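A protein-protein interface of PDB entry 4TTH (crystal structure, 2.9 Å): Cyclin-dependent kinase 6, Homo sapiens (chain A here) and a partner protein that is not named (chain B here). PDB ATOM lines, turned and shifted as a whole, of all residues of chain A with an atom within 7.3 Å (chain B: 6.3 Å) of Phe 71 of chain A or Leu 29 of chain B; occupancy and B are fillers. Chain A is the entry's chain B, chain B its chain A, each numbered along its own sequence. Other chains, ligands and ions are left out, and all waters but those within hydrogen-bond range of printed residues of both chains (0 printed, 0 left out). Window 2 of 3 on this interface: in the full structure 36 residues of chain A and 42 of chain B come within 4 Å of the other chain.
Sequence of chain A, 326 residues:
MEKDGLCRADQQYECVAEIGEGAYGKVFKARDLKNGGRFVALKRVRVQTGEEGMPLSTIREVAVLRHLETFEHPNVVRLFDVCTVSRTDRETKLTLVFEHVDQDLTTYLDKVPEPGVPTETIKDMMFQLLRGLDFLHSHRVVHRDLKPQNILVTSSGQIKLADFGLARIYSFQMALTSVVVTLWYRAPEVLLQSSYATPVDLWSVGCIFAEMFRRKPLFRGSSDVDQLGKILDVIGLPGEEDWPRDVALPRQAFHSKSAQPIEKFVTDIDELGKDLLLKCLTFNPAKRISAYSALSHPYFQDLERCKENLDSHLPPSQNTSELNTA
Of the 10 printed residues of chain A, 5 touch a printed residue of chain B.
Printed residues of chain A that touch a printed residue of chain B: His 67, Leu 68, Thr 70, Phe 71 and His 139.
Printed residues of chain B that touch a printed residue of chain A: Asn 26, Leu 29, Arg 30 and Leu 33.
Hydrophobic or aromatic side chains of chain B that line the printed part of chain A: Leu 29 and Leu 33.
Along chain B the printed residues that touch a printed residue of chain A span positions 26 to 33.
Among the printed residues, 8 pairs touch across the chains.
Among the printed residues, no Asp or Glu carboxylate lies within 4 Å of a Lys or Arg side-chain nitrogen of the other chain.
His 67 of chain A touches Leu 33 of chain B.
Leu 68 of chain A touches Arg 30 of chain B.
Thr 70 of chain A touches Leu 33 of chain B (OG1 to CD1, 3.7 Å).
CZ of Phe 71 of chain A touches CD2 of Leu 29 of chain B, 3.6 Å away.
Arg 30 of chain B touches Phe 71 of chain A (CG to CE2, 3.7 Å).
Phe 71 of chain A touches just these residues of chain B: Leu 29 (3.6 Å) and Arg 30 (3.7 Å).
Of the printed residues of chain A, Leu 29 of chain B touches Phe 71 (3.6 Å).
Of the printed residues of chain B, Leu 68 of chain A touches Arg 30.
Printed residues of chain B within 4 Å of His 67 of chain A: Arg 30 and Leu 33.
The nearest residue of chain A that does not touch Leu 29 of chain B is His 139 of chain A (5.7 Å).
A ring nitrogen (NE2) of His 139 of chain A lies close to the side-chain amide nitrogen (ND2) of Asn 26 of chain B (3.2 Å).
The guanidinium group of Arg 30 of chain B sits at hydrogen-bond distance from a ring nitrogen (NE2) of His 67 of chain A (2.9 Å).
A ring nitrogen (ND1) of His 139 of chain A sits close to the guanidinium group of Arg 30 of chain B, at 3.5 Å.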
ATOM      1  N   HIS A  67      19.842  10.432   6.383  1.00  0.00           N
ATOM      2  CA  HIS A  67      19.489   9.298   5.550  1.00  0.00           C
ATOM      3  C   HIS A  67      18.156   9.628   4.943  1.00  0.00           C
ATOM      4  O   HIS A  67      17.875   9.294   3.800  1.00  0.00           O
ATOM      5  CB  HIS A  67      19.422   7.979   6.362  1.00  0.00           C
ATOM      6  CG  HIS A  67      19.115   6.767   5.527  1.00  0.00           C
ATOM      7  ND1 HIS A  67      19.818   6.453   4.383  1.00  0.00           N
ATOM      8  CD2 HIS A  67      18.176   5.802   5.667  1.00  0.00           C
ATOM      9  CE1 HIS A  67      19.324   5.346   3.856  1.00  0.00           C
ATOM     10  NE2 HIS A  67      18.326   4.931   4.614  1.00  0.00           N
ATOM     11  N   LEU A  68      17.337  10.303   5.731  1.00  0.00           N
ATOM     12  CA  LEU A  68      15.945  10.489   5.387  1.00  0.00           C
ATOM     13  C   LEU A  68      15.655  11.904   4.881  1.00  0.00           C
ATOM     14  O   LEU A  68      14.557  12.182   4.409  1.00  0.00           O
ATOM     15  CB  LEU A  68      15.066  10.140   6.593  1.00  0.00           C
ATOM     16  CG  LEU A  68      15.007   8.647   6.921  1.00  0.00           C
ATOM     17  CD1 LEU A  68      13.797   8.263   7.774  1.00  0.00           C
ATOM     18  CD2 LEU A  68      15.018   7.849   5.641  1.00  0.00           C
ATOM     19  N   GLU A  69      16.656  12.776   4.933  1.00  0.00           N
ATOM     20  CA  GLU A  69      16.430  14.200   4.725  1.00  0.00           C
ATOM     21  C   GLU A  69      15.874  14.620   3.375  1.00  0.00           C
ATOM     22  O   GLU A  69      15.084  15.564   3.309  1.00  0.00           O
ATOM     23  CB  GLU A  69      17.681  15.007   5.045  1.00  0.00           C
ATOM     24  CG  GLU A  69      18.875  14.688   4.214  1.00  0.00           C
ATOM     25  CD  GLU A  69      20.087  15.430   4.730  1.00  0.00           C
ATOM     26  OE1 GLU A  69      21.092  15.537   3.992  1.00  0.00           O
ATOM     27  OE2 GLU A  69      20.021  15.914   5.887  1.00  0.00           O
ATOM     28  N   THR A  70      16.267  13.931   2.307  1.00  0.00           N
ATOM     29  CA  THR A  70      15.794  14.318   0.980  1.00  0.00           C
ATOM     30  C   THR A  70      14.296  14.122   0.850  1.00  0.00           C
ATOM     31  O   THR A  70      13.676  14.682  -0.053  1.00  0.00           O
ATOM     32  CB  THR A  70      16.471  13.543  -0.169  1.00  0.00           C
ATOM     33  OG1 THR A  70      15.989  12.195  -0.203  1.00  0.00           O
ATOM     34  CG2 THR A  70      17.972  13.573  -0.041  1.00  0.00           C
ATOM     35  N   PHE A  71      13.712  13.322   1.734  1.00  0.00           N
ATOM     36  CA  PHE A  71      12.264  13.142   1.755  1.00  0.00           C
ATOM     37  C   PHE A  71      11.577  14.396   2.267  1.00  0.00           C
ATOM     38  O   PHE A  71      10.353  14.495   2.191  1.00  0.00           O
ATOM     39  CB  PHE A  71      11.874  12.008   2.685  1.00  0.00           C
ATOM     40  CG  PHE A  71      11.916  10.659   2.062  1.00  0.00           C
ATOM     41  CD1 PHE A  71      10.796  10.150   1.421  1.00  0.00           C
ATOM     42  CD2 PHE A  71      13.049   9.868   2.167  1.00  0.00           C
ATOM     43  CE1 PHE A  71      10.810   8.893   0.865  1.00  0.00           C
ATOM     44  CE2 PHE A  71      13.074   8.609   1.616  1.00  0.00           C
ATOM     45  CZ  PHE A  71      11.957   8.118   0.960  1.00  0.00           C
ATOM     46  N   GLU A  72      12.366  15.325   2.811  1.00  0.00           N
ATOM     47  CA  GLU A  72      11.866  16.569   3.404  1.00  0.00           C
ATOM     48  C   GLU A  72      10.497  16.446   4.092  1.00  0.00           C
ATOM     49  O   GLU A  72       9.532  17.040   3.646  1.00  0.00           O
ATOM     50  CB  GLU A  72      11.825  17.682   2.352  1.00  0.00           C
ATOM     51  CG  GLU A  72      13.188  18.098   1.807  1.00  0.00           C
ATOM     52  CD  GLU A  72      13.103  18.925   0.519  1.00  0.00           C
ATOM     53  OE1 GLU A  72      12.203  18.675  -0.321  1.00  0.00           O
ATOM     54  OE2 GLU A  72      13.951  19.828   0.344  1.00  0.00           O
ATOM     55  N   HIS A  73      10.404  15.670   5.168  1.00  0.00           N
ATOM     56  CA  HIS A  73       9.131  15.533   5.873  1.00  0.00           C
ATOM     57  C   HIS A  73       8.890  16.740   6.761  1.00  0.00           C
ATOM     58  O   HIS A  73       9.796  17.186   7.466  1.00  0.00           O
ATOM     59  CB  HIS A  73       9.067  14.250   6.695  1.00  0.00           C
ATOM     60  CG  HIS A  73       7.686  13.888   7.133  1.00  0.00           C
ATOM     61  ND1 HIS A  73       7.065  14.493   8.205  1.00  0.00           N
ATOM     62  CD2 HIS A  73       6.799  12.990   6.644  1.00  0.00           C
ATOM     63  CE1 HIS A  73       5.856  13.980   8.352  1.00  0.00           C
ATOM     64  NE2 HIS A  73       5.672  13.061   7.422  1.00  0.00           N
ATOM     65  N   PRO A  74       7.665  17.294   6.690  1.00  0.00           N
ATOM     66  CA  PRO A  74       7.190  18.467   7.428  1.00  0.00           C
ATOM     67  C   PRO A  74       7.534  18.379   8.908  1.00  0.00           C
ATOM     68  O   PRO A  74       7.799  19.393   9.563  1.00  0.00           O
ATOM     69  CB  PRO A  74       5.681  18.354   7.295  1.00  0.00           C
ATOM     70  CG  PRO A  74       5.445  17.589   6.045  1.00  0.00           C
ATOM     71  CD  PRO A  74       6.638  16.767   5.763  1.00  0.00           C
ATOM     72  N   PHE A 135       5.746   8.425   9.128  1.00  0.00           N
ATOM     73  CA  PHE A 135       6.919   8.610   8.295  1.00  0.00           C
ATOM     74  C   PHE A 135       7.987   7.642   8.728  1.00  0.00           C
ATOM     75  O   PHE A 135       8.158   6.576   8.131  1.00  0.00           O
ATOM     76  CB  PHE A 135       7.458  10.020   8.484  1.00  0.00           C
ATOM     77  CG  PHE A 135       8.703  10.302   7.702  1.00  0.00           C
ATOM     78  CD1 PHE A 135       8.777   9.984   6.357  1.00  0.00           C
ATOM     79  CD2 PHE A 135       9.784  10.917   8.293  1.00  0.00           C
ATOM     80  CE1 PHE A 135       9.917  10.259   5.618  1.00  0.00           C
ATOM     81  CE2 PHE A 135      10.929  11.188   7.566  1.00  0.00           C
ATOM     82  CZ  PHE A 135      10.988  10.857   6.219  1.00  0.00           C
ATOM     83  N   HIS A 139      10.075   3.792   7.453  1.00  0.00           N
ATOM     84  CA  HIS A 139      11.480   3.697   7.094  1.00  0.00           C
ATOM     85  C   HIS A 139      12.268   2.848   8.097  1.00  0.00           C
ATOM     86  O   HIS A 139      13.500   2.931   8.197  1.00  0.00           O
ATOM     87  CB  HIS A 139      12.040   5.092   6.908  1.00  0.00           C
ATOM     88  CG  HIS A 139      11.450   5.782   5.713  1.00  0.00           C
ATOM     89  ND1 HIS A 139      11.813   5.462   4.421  1.00  0.00           N
ATOM     90  CD2 HIS A 139      10.467   6.706   5.609  1.00  0.00           C
ATOM     91  CE1 HIS A 139      11.114   6.193   3.577  1.00  0.00           C
ATOM     92  NE2 HIS A 139      10.290   6.956   4.273  1.00  0.00           N
ATOM     93  N   LEU B  24       8.686  -2.210   2.089  1.00  0.00           N
ATOM     94  CA  LEU B  24       9.365  -2.770   0.946  1.00  0.00           C
ATOM     95  C   LEU B  24       9.492  -1.710  -0.135  1.00  0.00           C
ATOM     96  O   LEU B  24      10.560  -1.563  -0.727  1.00  0.00           O
ATOM     97  CB  LEU B  24       8.601  -3.965   0.409  1.00  0.00           C
ATOM     98  CG  LEU B  24       9.372  -4.727  -0.661  1.00  0.00           C
ATOM     99  CD1 LEU B  24      10.836  -4.778  -0.316  1.00  0.00           C
ATOM    100  CD2 LEU B  24       8.826  -6.126  -0.804  1.00  0.00           C
ATOM    101  N   ASN B  25       8.394  -0.984  -0.381  1.00  0.00           N
ATOM    102  CA  ASN B  25       8.400   0.149  -1.287  1.00  0.00           C
ATOM    103  C   ASN B  25       9.523   1.112  -0.933  1.00  0.00           C
ATOM    104  O   ASN B  25      10.382   1.392  -1.764  1.00  0.00           O
ATOM    105  CB  ASN B  25       7.051   0.894  -1.286  1.00  0.00           C
ATOM    106  CG  ASN B  25       5.913   0.097  -1.961  1.00  0.00           C
ATOM    107  OD1 ASN B  25       6.159  -0.903  -2.645  1.00  0.00           O
ATOM    108  ND2 ASN B  25       4.660   0.554  -1.768  1.00  0.00           N
ATOM    109  N   ASN B  26       9.530   1.617   0.298  1.00  0.00           N
ATOM    110  CA  ASN B  26      10.505   2.645   0.680  1.00  0.00           C
ATOM    111  C   ASN B  26      11.941   2.152   0.719  1.00  0.00           C
ATOM    112  O   ASN B  26      12.871   2.950   0.744  1.00  0.00           O
ATOM    113  CB  ASN B  26      10.168   3.269   2.034  1.00  0.00           C
ATOM    114  CG  ASN B  26       8.797   3.882   2.070  1.00  0.00           C
ATOM    115  OD1 ASN B  26       8.028   3.762   1.122  1.00  0.00           O
ATOM    116  ND2 ASN B  26       8.473   4.532   3.177  1.00  0.00           N
ATOM    117  N   LEU B  27      12.121   0.837   0.765  1.00  0.00           N
ATOM    118  CA  LEU B  27      13.460   0.265   0.736  1.00  0.00           C
ATOM    119  C   LEU B  27      13.991   0.393  -0.683  1.00  0.00           C
ATOM    120  O   LEU B  27      15.074   0.952  -0.903  1.00  0.00           O
ATOM    121  CB  LEU B  27      13.447  -1.198   1.189  1.00  0.00           C
ATOM    122  CG  LEU B  27      13.582  -1.525   2.680  1.00  0.00           C
ATOM    123  CD1 LEU B  27      13.316  -2.987   2.921  1.00  0.00           C
ATOM    124  CD2 LEU B  27      14.947  -1.157   3.145  1.00  0.00           C
ATOM    125  N   LYS B  28      13.202  -0.129  -1.628  1.00  0.00           N
ATOM    126  CA  LYS B  28      13.337   0.115  -3.072  1.00  0.00           C
ATOM    127  C   LYS B  28      13.701   1.560  -3.413  1.00  0.00           C
ATOM    128  O   LYS B  28      14.524   1.818  -4.281  1.00  0.00           O
ATOM    129  CB  LYS B  28      12.029  -0.258  -3.755  1.00  0.00           C
ATOM    130  CG  LYS B  28      12.039  -1.613  -4.395  1.00  0.00           C
ATOM    131  CD  LYS B  28      10.814  -2.436  -4.067  1.00  0.00           C
ATOM    132  CE  LYS B  28       9.614  -2.050  -4.915  1.00  0.00           C
ATOM    133  NZ  LYS B  28       9.489  -2.873  -6.132  1.00  0.00           N
ATOM    134  N   LEU B  29      13.080   2.502  -2.722  1.00  0.00           N
ATOM    135  CA  LEU B  29      13.357   3.903  -2.935  1.00  0.00           C
ATOM    136  C   LEU B  29      14.732   4.298  -2.458  1.00  0.00           C
ATOM    137  O   LEU B  29      15.592   4.635  -3.245  1.00  0.00           O
ATOM    138  CB  LEU B  29      12.333   4.734  -2.184  1.00  0.00           C
ATOM    139  CG  LEU B  29      11.348   5.551  -3.007  1.00  0.00           C
ATOM    140  CD1 LEU B  29      10.225   4.665  -3.546  1.00  0.00           C
ATOM    141  CD2 LEU B  29      10.827   6.672  -2.138  1.00  0.00           C
ATOM    142  N   ARG B  30      14.942   4.248  -1.150  1.00  0.00           N
ATOM    143  CA  ARG B  30      16.188   4.728  -0.548  1.00  0.00           C
ATOM    144  C   ARG B  30      17.411   3.944  -1.024  1.00  0.00           C
ATOM    145  O   ARG B  30      18.542   4.406  -0.906  1.00  0.00           O
ATOM    146  CB  ARG B  30      16.070   4.750   0.975  1.00  0.00           C
ATOM    147  CG  ARG B  30      14.709   5.239   1.461  1.00  0.00           C
ATOM    148  CD  ARG B  30      14.668   5.472   2.968  1.00  0.00           C
ATOM    149  NE  ARG B  30      15.613   4.598   3.649  1.00  0.00           N
ATOM    150  CZ  ARG B  30      15.346   3.391   4.136  1.00  0.00           C
ATOM    151  NH1 ARG B  30      14.124   2.861   4.078  1.00  0.00           N
ATOM    152  NH2 ARG B  30      16.337   2.722   4.691  1.00  0.00           N
ATOM    153  N   GLU B  31      17.161   2.761  -1.571  1.00  0.00           N
ATOM    154  CA  GLU B  31      18.148   2.027  -2.348  1.00  0.00           C
ATOM    155  C   GLU B  31      18.670   2.908  -3.498  1.00  0.00           C
ATOM    156  O   GLU B  31      19.846   2.826  -3.866  1.00  0.00           O
ATOM    157  CB  GLU B  31      17.517   0.740  -2.896  1.00  0.00           C
ATOM    158  CG  GLU B  31      18.477  -0.286  -3.484  1.00  0.00           C
ATOM    159  CD  GLU B  31      17.752  -1.538  -4.018  1.00  0.00           C
ATOM    160  OE1 GLU B  31      18.419  -2.565  -4.277  1.00  0.00           O
ATOM    161  OE2 GLU B  31      16.512  -1.507  -4.191  1.00  0.00           O
ATOM    162  N   LEU B  32      17.807   3.760  -4.057  1.00  0.00           N
ATOM    163  CA  LEU B  32      18.229   4.668  -5.131  1.00  0.00           C
ATOM    164  C   LEU B  32      18.959   5.924  -4.612  1.00  0.00           C
ATOM    165  O   LEU B  32      19.337   6.796  -5.385  1.00  0.00           O
ATOM    166  CB  LEU B  32      17.050   5.055  -6.029  1.00  0.00           C
ATOM    167  CG  LEU B  32      16.083   3.959  -6.508  1.00  0.00           C
ATOM    168  CD1 LEU B  32      14.758   4.587  -6.916  1.00  0.00           C
ATOM    169  CD2 LEU B  32      16.642   3.117  -7.661  1.00  0.00           C
ATOM    170  N   LEU B  33      19.184   5.998  -3.304  1.00  0.00           N
ATOM    171  CA  LEU B  33      19.945   7.105  -2.718  1.00  0.00           C
ATOM    172  C   LEU B  33      21.432   6.804  -2.523  1.00  0.00           C
ATOM    173  O   LEU B  33      22.191   7.682  -2.113  1.00  0.00           O
ATOM    174  CB  LEU B  33      19.338   7.548  -1.381  1.00  0.00           C
ATOM    175  CG  LEU B  33      18.115   8.458  -1.494  1.00  0.00           C
ATOM    176  CD1 LEU B  33      17.603   8.850  -0.105  1.00  0.00           C
ATOM    177  CD2 LEU B  33      18.466   9.683  -2.323  1.00  0.00           C
ATOM    178  N   VAL B 150      21.219   1.596   2.773  1.00  0.00           N
ATOM    179  CA  VAL B 150      20.291   0.507   2.685  1.00  0.00           C
ATOM    180  C   VAL B 150      21.158  -0.722   2.513  1.00  0.00           C
ATOM    181  O   VAL B 150      21.951  -0.807   1.569  1.00  0.00           O
ATOM    182  CB  VAL B 150      19.289   0.699   1.532  1.00  0.00           C
ATOM    183  CG1 VAL B 150      18.538  -0.596   1.250  1.00  0.00           C
ATOM    184  CG2 VAL B 150      18.324   1.802   1.880  1.00  0.00           C
